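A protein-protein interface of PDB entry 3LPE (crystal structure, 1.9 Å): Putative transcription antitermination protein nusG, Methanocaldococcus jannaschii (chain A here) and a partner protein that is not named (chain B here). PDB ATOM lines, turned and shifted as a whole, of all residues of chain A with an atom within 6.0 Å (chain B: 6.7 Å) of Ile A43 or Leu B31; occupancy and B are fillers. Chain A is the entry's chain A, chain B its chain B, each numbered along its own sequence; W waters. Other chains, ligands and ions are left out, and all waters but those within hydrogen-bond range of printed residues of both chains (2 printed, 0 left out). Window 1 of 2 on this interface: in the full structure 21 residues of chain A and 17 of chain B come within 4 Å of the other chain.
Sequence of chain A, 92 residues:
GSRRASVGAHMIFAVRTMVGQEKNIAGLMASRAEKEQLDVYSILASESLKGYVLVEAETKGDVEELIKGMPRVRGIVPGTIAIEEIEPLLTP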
ATOM      1  N   ILE A  25      -3.867 -26.467  28.794  1.00  0.00           N
ATOM      2  CA  ILE A  25      -2.449 -26.387  29.106  1.00  0.00           C
ATOM      3  C   ILE A  25      -1.903 -24.936  29.002  1.00  0.00           C
ATOM      4  O   ILE A  25      -1.081 -24.522  29.801  1.00  0.00           O
ATOM      5  CB  ILE A  25      -1.642 -27.371  28.253  1.00  0.00           C
ATOM      6  CG1 ILE A  25      -1.792 -28.769  28.850  1.00  0.00           C
ATOM      7  CG2 ILE A  25      -0.171 -26.990  28.239  1.00  0.00           C
ATOM      8  CD1 ILE A  25      -1.688 -29.848  27.829  1.00  0.00           C
ATOM      9  N   ALA A  26      -2.386 -24.187  28.026  1.00  0.00           N
ATOM     10  CA  ALA A  26      -2.012 -22.773  27.902  1.00  0.00           C
ATOM     11  C   ALA A  26      -2.346 -22.038  29.209  1.00  0.00           C
ATOM     12  O   ALA A  26      -1.573 -21.208  29.653  1.00  0.00           O
ATOM     13  CB  ALA A  26      -2.754 -22.138  26.759  1.00  0.00           C
ATOM     14  N   GLY A  27      -3.504 -22.343  29.788  1.00  0.00           N
ATOM     15  CA  GLY A  27      -3.933 -21.754  31.051  1.00  0.00           C
ATOM     16  C   GLY A  27      -3.040 -22.085  32.238  1.00  0.00           C
ATOM     17  O   GLY A  27      -2.653 -21.204  33.007  1.00  0.00           O
ATOM     18  N   MET A  29       0.005 -23.068  31.960  1.00  0.00           N
ATOM     19  CA  MET A  29       1.301 -22.483  31.653  1.00  0.00           C
ATOM     20  C   MET A  29       1.349 -21.025  32.109  1.00  0.00           C
ATOM     21  O   MET A  29       2.320 -20.582  32.712  1.00  0.00           O
ATOM     22  CB  MET A  29       1.562 -22.537  30.151  1.00  0.00           C
ATOM     23  CG  MET A  29       2.092 -23.877  29.663  1.00  0.00           C
ATOM     24  SD  MET A  29       2.055 -23.888  27.882  1.00  0.00           S
ATOM     25  CE  MET A  29       3.255 -25.160  27.492  1.00  0.00           C
ATOM     26  N   ALA A  30       0.311 -20.275  31.791  1.00  0.00           N
ATOM     27  CA  ALA A  30       0.320 -18.837  32.110  1.00  0.00           C
ATOM     28  C   ALA A  30       0.408 -18.638  33.625  1.00  0.00           C
ATOM     29  O   ALA A  30       1.161 -17.806  34.117  1.00  0.00           O
ATOM     30  CB  ALA A  30      -0.915 -18.153  31.553  1.00  0.00           C
ATOM     31  N   ALA A  33       3.945 -19.531  34.734  1.00  0.00           N
ATOM     32  CA  ALA A  33       4.907 -18.541  34.278  1.00  0.00           C
ATOM     33  C   ALA A  33       4.920 -17.341  35.244  1.00  0.00           C
ATOM     34  O   ALA A  33       5.976 -16.874  35.641  1.00  0.00           O
ATOM     35  CB  ALA A  33       4.579 -18.095  32.852  1.00  0.00           C
ATOM     36  N   VAL A  40       8.515 -15.961  30.083  1.00  0.00           N
ATOM     37  CA  VAL A  40       7.567 -16.420  29.077  1.00  0.00           C
ATOM     38  C   VAL A  40       6.671 -15.229  28.757  1.00  0.00           C
ATOM     39  O   VAL A  40       6.092 -14.618  29.661  1.00  0.00           O
ATOM     40  CB  VAL A  40       6.723 -17.594  29.614  1.00  0.00           C
ATOM     41  CG1 VAL A  40       5.630 -17.988  28.623  1.00  0.00           C
ATOM     42  CG2 VAL A  40       7.610 -18.792  29.939  1.00  0.00           C
ATOM     43  N   TYR A  41       6.560 -14.895  27.476  1.00  0.00           N
ATOM     44  CA  TYR A  41       5.891 -13.667  27.079  1.00  0.00           C
ATOM     45  C   TYR A  41       4.505 -13.854  26.488  1.00  0.00           C
ATOM     46  O   TYR A  41       3.639 -12.993  26.642  1.00  0.00           O
ATOM     47  CB  TYR A  41       6.772 -12.908  26.103  1.00  0.00           C
ATOM     48  CG  TYR A  41       8.178 -12.729  26.608  1.00  0.00           C
ATOM     49  CD1 TYR A  41       8.421 -12.242  27.891  1.00  0.00           C
ATOM     50  CD2 TYR A  41       9.265 -13.013  25.799  1.00  0.00           C
ATOM     51  CE1 TYR A  41       9.722 -12.058  28.360  1.00  0.00           C
ATOM     52  CE2 TYR A  41      10.562 -12.830  26.250  1.00  0.00           C
ATOM     53  CZ  TYR A  41      10.790 -12.349  27.532  1.00  0.00           C
ATOM     54  OH  TYR A  41      12.083 -12.161  27.976  1.00  0.00           O
ATOM     55  N   SER A  42       4.286 -14.975  25.811  1.00  0.00           N
ATOM     56  CA  SER A  42       2.956 -15.263  25.298  1.00  0.00           C
ATOM     57  C   SER A  42       2.821 -16.754  25.036  1.00  0.00           C
ATOM     58  O   SER A  42       3.814 -17.454  24.954  1.00  0.00           O
ATOM     59  CB  SER A  42       2.626 -14.456  24.032  1.00  0.00           C
ATOM     60  OG  SER A  42       3.319 -14.971  22.909  1.00  0.00           O
ATOM     61  N   ILE A  43       1.575 -17.208  24.953  1.00  0.00           N
ATOM     62  CA  ILE A  43       1.251 -18.614  24.766  1.00  0.00           C
ATOM     63  C   ILE A  43       0.109 -18.644  23.772  1.00  0.00           C
ATOM     64  O   ILE A  43      -0.858 -17.905  23.907  1.00  0.00           O
ATOM     65  CB  ILE A  43       0.811 -19.272  26.081  1.00  0.00           C
ATOM     66  CG1 ILE A  43       1.910 -19.151  27.137  1.00  0.00           C
ATOM     67  CG2 ILE A  43       0.543 -20.772  25.889  1.00  0.00           C
ATOM     68  CD1 ILE A  43       1.363 -19.274  28.541  1.00  0.00           C
ATOM     69  N   LEU A  44       0.236 -19.460  22.734  1.00  0.00           N
ATOM     70  CA  LEU A  44      -0.761 -19.423  21.669  1.00  0.00           C
ATOM     71  C   LEU A  44      -1.297 -20.831  21.395  1.00  0.00           C
ATOM     72  O   LEU A  44      -0.515 -21.762  21.139  1.00  0.00           O
ATOM     73  CB  LEU A  44      -0.133 -18.824  20.394  1.00  0.00           C
ATOM     74  CG  LEU A  44      -0.900 -19.006  19.093  1.00  0.00           C
ATOM     75  CD1 LEU A  44      -2.004 -18.010  19.025  1.00  0.00           C
ATOM     76  CD2 LEU A  44       0.020 -18.863  17.905  1.00  0.00           C
ATOM     77  N   ALA A  45      -2.615 -20.979  21.469  1.00  0.00           N
ATOM     78  CA  ALA A  45      -3.271 -22.246  21.186  1.00  0.00           C
ATOM     79  C   ALA A  45      -4.248 -22.032  20.053  1.00  0.00           C
ATOM     80  O   ALA A  45      -5.309 -21.454  20.256  1.00  0.00           O
ATOM     81  CB  ALA A  45      -3.984 -22.793  22.428  1.00  0.00           C
ATOM     82  N   VAL A  53       0.951 -26.355  21.672  1.00  0.00           N
ATOM     83  CA  VAL A  53       0.802 -24.992  22.172  1.00  0.00           C
ATOM     84  C   VAL A  53       2.121 -24.295  21.854  1.00  0.00           C
ATOM     85  O   VAL A  53       3.203 -24.890  21.998  1.00  0.00           O
ATOM     86  CB  VAL A  53       0.511 -24.988  23.694  1.00  0.00           C
ATOM     87  CG1 VAL A  53       0.516 -23.583  24.244  1.00  0.00           C
ATOM     88  CG2 VAL A  53      -0.851 -25.635  23.961  1.00  0.00           C
ATOM     89  N   LEU A  54       2.043 -23.054  21.390  1.00  0.00           N
ATOM     90  CA  LEU A  54       3.247 -22.303  21.030  1.00  0.00           C
ATOM     91  C   LEU A  54       3.607 -21.385  22.180  1.00  0.00           C
ATOM     92  O   LEU A  54       2.739 -20.683  22.670  1.00  0.00           O
ATOM     93  CB  LEU A  54       2.958 -21.461  19.793  1.00  0.00           C
ATOM     94  CG  LEU A  54       2.608 -22.286  18.544  1.00  0.00           C
ATOM     95  CD1 LEU A  54       2.347 -21.395  17.343  1.00  0.00           C
ATOM     96  CD2 LEU A  54       3.703 -23.285  18.223  1.00  0.00           C
ATOM     97  N   VAL A  55       4.881 -21.371  22.583  1.00  0.00           N
ATOM     98  CA  VAL A  55       5.309 -20.615  23.761  1.00  0.00           C
ATOM     99  C   VAL A  55       6.429 -19.684  23.347  1.00  0.00           C
ATOM    100  O   VAL A  55       7.463 -20.124  22.891  1.00  0.00           O
ATOM    101  CB  VAL A  55       5.807 -21.543  24.903  1.00  0.00           C
ATOM    102  CG1 VAL A  55       6.315 -20.741  26.121  1.00  0.00           C
ATOM    103  CG2 VAL A  55       4.692 -22.532  25.335  1.00  0.00           C
ATOM    104  N   GLU A  56       6.187 -18.387  23.482  1.00  0.00           N
ATOM    105  CA  GLU A  56       7.205 -17.366  23.225  1.00  0.00           C
ATOM    106  C   GLU A  56       7.960 -17.078  24.538  1.00  0.00           C
ATOM    107  O   GLU A  56       7.363 -16.693  25.561  1.00  0.00           O
ATOM    108  CB  GLU A  56       6.524 -16.106  22.686  1.00  0.00           C
ATOM    109  CG  GLU A  56       7.473 -15.005  22.203  1.00  0.00           C
ATOM    110  CD  GLU A  56       6.735 -13.753  21.781  1.00  0.00           C
ATOM    111  OE1 GLU A  56       7.316 -12.945  21.035  1.00  0.00           O
ATOM    112  OE2 GLU A  56       5.572 -13.578  22.178  1.00  0.00           O
ATOM    113  N   LEU A  66       8.964 -24.252  32.495  1.00  0.00           N
ATOM    114  CA  LEU A  66       7.524 -24.031  32.396  1.00  0.00           C
ATOM    115  C   LEU A  66       6.771 -25.374  32.393  1.00  0.00           C
ATOM    116  O   LEU A  66       5.770 -25.540  33.090  1.00  0.00           O
ATOM    117  CB  LEU A  66       7.213 -23.238  31.112  1.00  0.00           C
ATOM    118  CG  LEU A  66       5.734 -22.964  30.836  1.00  0.00           C
ATOM    119  CD1 LEU A  66       5.199 -21.965  31.887  1.00  0.00           C
ATOM    120  CD2 LEU A  66       5.533 -22.440  29.427  1.00  0.00           C
ATOM    121  N   LEU A  90      -2.755 -16.131  13.501  1.00  0.00           N
ATOM    122  CA  LEU A  90      -3.323 -14.986  14.212  1.00  0.00           C
ATOM    123  C   LEU A  90      -4.684 -14.564  13.683  1.00  0.00           C
ATOM    124  O   LEU A  90      -5.547 -14.125  14.437  1.00  0.00           O
ATOM    125  CB  LEU A  90      -2.363 -13.803  14.174  1.00  0.00           C
ATOM    126  CG  LEU A  90      -1.508 -13.630  15.426  1.00  0.00           C
ATOM    127  CD1 LEU A  90      -1.272 -14.951  16.114  1.00  0.00           C
ATOM    128  CD2 LEU A  90      -0.188 -12.958  15.078  1.00  0.00           C
ATOM    129  N   LEU B  10     -10.748 -11.776  26.507  1.00  0.00           N
ATOM    130  CA  LEU B  10     -11.598 -12.824  27.077  1.00  0.00           C
ATOM    131  C   LEU B  10     -12.043 -12.494  28.482  1.00  0.00           C
ATOM    132  O   LEU B  10     -11.218 -12.124  29.307  1.00  0.00           O
ATOM    133  CB  LEU B  10     -10.839 -14.147  27.105  1.00  0.00           C
ATOM    134  CG  LEU B  10     -10.529 -14.717  25.722  1.00  0.00           C
ATOM    135  CD1 LEU B  10      -9.650 -15.943  25.942  1.00  0.00           C
ATOM    136  CD2 LEU B  10     -11.812 -15.154  25.067  1.00  0.00           C
ATOM    137  N   GLY B  29      -9.906 -19.934  19.355  1.00  0.00           N
ATOM    138  CA  GLY B  29      -8.479 -19.749  19.440  1.00  0.00           C
ATOM    139  C   GLY B  29      -8.139 -19.051  20.730  1.00  0.00           C
ATOM    140  O   GLY B  29      -8.981 -18.361  21.272  1.00  0.00           O
ATOM    141  N   LEU B  30      -6.910 -19.219  21.208  1.00  0.00           N
ATOM    142  CA  LEU B  30      -6.495 -18.616  22.472  1.00  0.00           C
ATOM    143  C   LEU B  30      -5.083 -18.054  22.367  1.00  0.00           C
ATOM    144  O   LEU B  30      -4.142 -18.760  21.974  1.00  0.00           O
ATOM    145  CB  LEU B  30      -6.577 -19.640  23.610  1.00  0.00           C
ATOM    146  CG  LEU B  30      -5.991 -19.251  24.969  1.00  0.00           C
ATOM    147  CD1 LEU B  30      -6.687 -18.004  25.489  1.00  0.00           C
ATOM    148  CD2 LEU B  30      -6.169 -20.408  25.957  1.00  0.00           C
ATOM    149  N   LEU B  31      -4.939 -16.776  22.693  1.00  0.00           N
ATOM    150  CA  LEU B  31      -3.619 -16.136  22.766  1.00  0.00           C
ATOM    151  C   LEU B  31      -3.513 -15.476  24.126  1.00  0.00           C
ATOM    152  O   LEU B  31      -4.270 -14.542  24.429  1.00  0.00           O
ATOM    153  CB  LEU B  31      -3.450 -15.090  21.657  1.00  0.00           C
ATOM    154  CG  LEU B  31      -2.199 -14.186  21.757  1.00  0.00           C
ATOM    155  CD1 LEU B  31      -0.917 -14.995  21.910  1.00  0.00           C
ATOM    156  CD2 LEU B  31      -2.078 -13.243  20.567  1.00  0.00           C
ATOM    157  N   ILE B  32      -2.600 -15.969  24.952  1.00  0.00           N
ATOM    158  CA  ILE B  32      -2.430 -15.417  26.281  1.00  0.00           C
ATOM    159  C   ILE B  32      -1.196 -14.556  26.230  1.00  0.00           C
ATOM    160  O   ILE B  32      -0.098 -15.063  25.993  1.00  0.00           O
ATOM    161  CB  ILE B  32      -2.201 -16.496  27.338  1.00  0.00           C
ATOM    162  CG1 ILE B  32      -3.401 -17.448  27.408  1.00  0.00           C
ATOM    163  CG2 ILE B  32      -1.952 -15.870  28.704  1.00  0.00           C
ATOM    164  CD1 ILE B  32      -3.195 -18.567  28.398  1.00  0.00           C
ATOM    165  N   VAL B  33      -1.386 -13.249  26.426  1.00  0.00           N
ATOM    166  CA  VAL B  33      -0.264 -12.338  26.449  1.00  0.00           C
ATOM    167  C   VAL B  33       0.138 -12.037  27.883  1.00  0.00           C
ATOM    168  O   VAL B  33      -0.601 -11.393  28.633  1.00  0.00           O
ATOM    169  CB  VAL B  33      -0.600 -11.032  25.715  1.00  0.00           C
ATOM    170  CG1 VAL B  33       0.605 -10.083  25.749  1.00  0.00           C
ATOM    171  CG2 VAL B  33      -1.019 -11.370  24.287  1.00  0.00           C
ATOM    172  N   ILE B  34       1.316 -12.496  28.263  1.00  0.00           N
ATOM    173  CA  ILE B  34       1.795 -12.292  29.616  1.00  0.00           C
ATOM    174  C   ILE B  34       2.584 -10.981  29.700  1.00  0.00           C
ATOM    175  O   ILE B  34       2.457 -10.226  30.657  1.00  0.00           O
ATOM    176  CB  ILE B  34       2.676 -13.473  30.052  1.00  0.00           C
ATOM    177  CG1 ILE B  34       1.851 -14.776  30.018  1.00  0.00           C
ATOM    178  CG2 ILE B  34       3.215 -13.249  31.438  1.00  0.00           C
ATOM    179  CD1 ILE B  34       2.676 -16.017  30.217  1.00  0.00           C
ATOM    180  N   SER B  39       6.534  -9.238  23.931  1.00  0.00           N
ATOM    181  CA  SER B  39       6.000 -10.254  23.024  1.00  0.00           C
ATOM    182  C   SER B  39       5.897  -9.774  21.566  1.00  0.00           C
ATOM    183  O   SER B  39       5.140  -8.856  21.250  1.00  0.00           O
ATOM    184  CB  SER B  39       4.645 -10.761  23.530  1.00  0.00           C
ATOM    185  OG  SER B  39       4.021 -11.564  22.564  1.00  0.00           O
ATOM    186  N   ILE B  41       4.687 -11.759  19.219  1.00  0.00           N
ATOM    187  CA  ILE B  41       3.366 -12.230  18.811  1.00  0.00           C
ATOM    188  C   ILE B  41       2.249 -11.233  19.193  1.00  0.00           C
ATOM    189  O   ILE B  41       1.352 -10.959  18.393  1.00  0.00           O
ATOM    190  CB  ILE B  41       3.051 -13.643  19.401  1.00  0.00           C
ATOM    191  CG1 ILE B  41       4.079 -14.662  18.900  1.00  0.00           C
ATOM    192  CG2 ILE B  41       1.630 -14.070  19.038  1.00  0.00           C
ATOM    193  CD1 ILE B  41       3.950 -16.061  19.531  1.00  0.00           C
ATOM    194  N   ALA B  42       2.293 -10.700  20.416  1.00  0.00           N
ATOM    195  CA  ALA B  42       1.299  -9.700  20.829  1.00  0.00           C
ATOM    196  C   ALA B  42       1.316  -8.517  19.858  1.00  0.00           C
ATOM    197  O   ALA B  42       0.272  -8.033  19.430  1.00  0.00           O
ATOM    198  CB  ALA B  42       1.582  -9.208  22.267  1.00  0.00           C
ATOM    199  N   ALA B  45      -0.323  -9.249  16.767  1.00  0.00           N
ATOM    200  CA  ALA B  45      -1.766  -9.371  16.996  1.00  0.00           C
ATOM    201  C   ALA B  45      -2.435  -8.042  17.345  1.00  0.00           C
ATOM    202  O   ALA B  45      -3.647  -7.996  17.524  1.00  0.00           O
ATOM    203  CB  ALA B  45      -2.072 -10.440  18.067  1.00  0.00           C
ATOM    204  N   ILE B  47      -1.910  -6.390  20.120  1.00  0.00           N
ATOM    205  CA  ILE B  47      -2.259  -6.418  21.535  1.00  0.00           C
ATOM    206  C   ILE B  47      -1.208  -5.665  22.347  1.00  0.00           C
ATOM    207  O   ILE B  47      -0.034  -5.975  22.261  1.00  0.00           O
ATOM    208  CB  ILE B  47      -2.321  -7.866  22.051  1.00  0.00           C
ATOM    209  CG1 ILE B  47      -3.466  -8.620  21.364  1.00  0.00           C
ATOM    210  CG2 ILE B  47      -2.476  -7.870  23.554  1.00  0.00           C
ATOM    211  CD1 ILE B  47      -3.458 -10.123  21.614  1.00  0.00           C
ATOM    212  N   GLY B  51      -3.297 -10.085  29.045  1.00  0.00           N
ATOM    213  CA  GLY B  51      -4.580 -10.728  29.188  1.00  0.00           C
ATOM    214  C   GLY B  51      -4.690 -11.921  28.260  1.00  0.00           C
ATOM    215  O   GLY B  51      -3.753 -12.291  27.578  1.00  0.00           O
ATOM    216  N   LYS B  52      -5.858 -12.527  28.234  1.00  0.00           N
ATOM    217  CA  LYS B  52      -6.089 -13.624  27.334  1.00  0.00           C
ATOM    218  C   LYS B  52      -7.039 -13.120  26.261  1.00  0.00           C
ATOM    219  O   LYS B  52      -7.964 -12.379  26.561  1.00  0.00           O
ATOM    220  CB  LYS B  52      -6.691 -14.802  28.116  1.00  0.00           C
ATOM    221  CG  LYS B  52      -5.908 -15.121  29.401  1.00  0.00           C
ATOM    222  CD  LYS B  52      -6.774 -15.851  30.422  1.00  0.00           C
ATOM    223  CE  LYS B  52      -6.532 -17.351  30.392  1.00  0.00           C
ATOM    224  NZ  LYS B  52      -5.275 -17.676  31.117  1.00  0.00           N
ATOM    225  N   TYR B  53      -6.806 -13.541  25.019  1.00  0.00           N
ATOM    226  CA  TYR B  53      -7.579 -13.114  23.865  1.00  0.00           C
ATOM    227  C   TYR B  53      -7.977 -14.294  22.984  1.00  0.00           C
ATOM    228  O   TYR B  53      -7.213 -15.266  22.838  1.00  0.00           O
ATOM    229  CB  TYR B  53      -6.743 -12.159  23.003  1.00  0.00           C
ATOM    230  CG  TYR B  53      -6.352 -10.894  23.729  1.00  0.00           C
ATOM    231  CD1 TYR B  53      -7.061  -9.720  23.537  1.00  0.00           C
ATOM    232  CD2 TYR B  53      -5.267 -10.878  24.595  1.00  0.00           C
ATOM    233  CE1 TYR B  53      -6.696  -8.540  24.203  1.00  0.00           C
ATOM    234  CE2 TYR B  53      -4.906  -9.715  25.271  1.00  0.00           C
ATOM    235  CZ  TYR B  53      -5.628  -8.552  25.063  1.00  0.00           C
ATOM    236  OH  TYR B  53      -5.271  -7.398  25.723  1.00  0.00           O
ATOM    237  N   ALA B  54      -9.137 -14.177  22.348  1.00  0.00           N
ATOM    238  CA  ALA B  54      -9.547 -15.163  21.343  1.00  0.00           C
ATOM    239  C   ALA B  54      -8.806 -14.832  20.058  1.00  0.00           C
ATOM    240  O   ALA B  54      -8.288 -13.720  19.936  1.00  0.00           O
ATOM    241  CB  ALA B  54     -11.061 -15.107  21.148  1.00  0.00           C
ATOM    242  N   LEU B  55      -8.705 -15.778  19.113  1.00  0.00           N
ATOM    243  CA  LEU B  55      -8.116 -15.460  17.816  1.00  0.00           C
ATOM    244  C   LEU B  55      -9.143 -14.918  16.833  1.00  0.00           C
ATOM    245  O   LEU B  55      -8.823 -14.131  15.946  1.00  0.00           O
ATOM    246  CB  LEU B  55      -7.382 -16.666  17.215  1.00  0.00           C
ATOM    247  CG  LEU B  55      -6.212 -17.136  18.068  1.00  0.00           C
ATOM    248  CD1 LEU B  55      -5.532 -18.334  17.408  1.00  0.00           C
ATOM    249  CD2 LEU B  55      -5.223 -15.992  18.277  1.00  0.00           C
HETATM  250  O   HOH W   1      -4.093 -18.818  33.484  1.00  0.00           O
HETATM  251  O   HOH W   2      -6.059 -12.678  16.366  1.00  0.00           O
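The backbone NH (N) of Val B33 sits at hydrogen-bond distance from the backbone carbonyl oxygen (O) of Gly B51 (2.8 Å). O of Gly B29 is in hydrogen-bond range of N of Leu B55 (3.4 Å). The side-chain hydroxyl (OG) of Ser B39 is in hydrogen-bond range of the backbone NH (N) of Ala B42, at 2.9 Å. OE2 of Glu A56 lies within hydrogen-bond range of OG of Ser A42 (2.7 Å). The backbone carbonyl oxygen of Glu A56 sits at hydrogen-bond distance from the backbone NH of Tyr A41 (2.7 Å). The backbone NH (N) of Leu A44 sits at hydrogen-bond distance from the backbone carbonyl oxygen (O) of Leu A54, at 2.8 Å.
OG of Ser B39 sits at hydrogen-bond distance from OG of Ser A42. N of Ile B34 sits at hydrogen-bond distance from O of Tyr A41 (2.9 Å). The backbone NH of Ala A45 is in hydrogen-bond range of the backbone carbonyl oxygen of Leu B30 (2.7 Å). OG of Ser B39 lies within hydrogen-bond range of OE2 of Glu A56, 2.6 Å away. O of Ile A43 sits at hydrogen-bond distance from N of Ile B32 (2.8 Å). The side-chain carboxylate (OE1) of Glu A56 lies within hydrogen-bond range of the backbone NH (N) of Ile B41 (3.4 Å).
CB of Ala A26 touches CD2 of Leu B30 (3.9 Å). Ala A26 touches Ile B32. CG2 of Ile B32 touches CB of Ala A30 (3.8 Å). Ile B34 touches Ala A33 (CD1 to CB, 3.9 Å). O of Tyr A41 touches C of Val B33, at 3.8 Å. Tyr A41 touches Ser B39 (O to CB, 3.96 Å). Ser A42 touches Ile B41. Ile B34 touches Ile A43. CA of Leu A44 touches O of Leu B30 (3.5 Å). O of Ala A45 touches CA of Gly B29 (3.7 Å).
Of the 18 printed residues of chain A, 11 touch a printed residue of chain B. Hydrophobic or aromatic side chains of chain A within 4 Å of the printed part of chain B: Ala A26, Ala A30, Ala A33, Val A40, Tyr A41, Ile A43 and Leu A44. Along chain A the printed residues that touch a printed residue of chain B span positions 26 to 90. Of the 17 printed residues of chain B, 9 touch a printed residue of chain A. Hydrophobic or aromatic side chains of chain B that line the printed part of chain A: Leu B30, Leu B31, Ile B32, Ile B34, Ile B41 and Leu B55. Among the printed residues, 22 pairs touch across the chains. Among the printed residues, no Asp or Glu carboxylate lies within 4 Å of a Lys or Arg side-chain nitrogen of the other chain.
Water W2 lies within hydrogen-bond range of the backbone carbonyl oxygen of Leu A90 and the backbone carbonyl oxygen of Leu B55. Water W1 bridges the backbone carbonyl oxygen (O) of Gly A27 (2.8 Å) and the side-chain amino group (NZ) of Lys B52 (2.9 Å).
Ile A25 touches none of the printed residues of chain B. Printed residues of chain B within 4 Å of Ala A26: Leu B30 and Ile B32. Of the printed residues of chain B, Ala A33 touches Ile B34. Printed residues of chain B within 4 Å of Val A40: Ile B34. Printed residues of chain B within 4 Å of Leu A44: Leu B30 (3.5 Å) and Leu B55 (3.9 Å). Printed residues of chain A within 4 Å of Gly B29: Ala A45 (3.7 Å). Of chain A, only Ile A43 (3.5 Å) comes within 4 Å of Leu B31.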
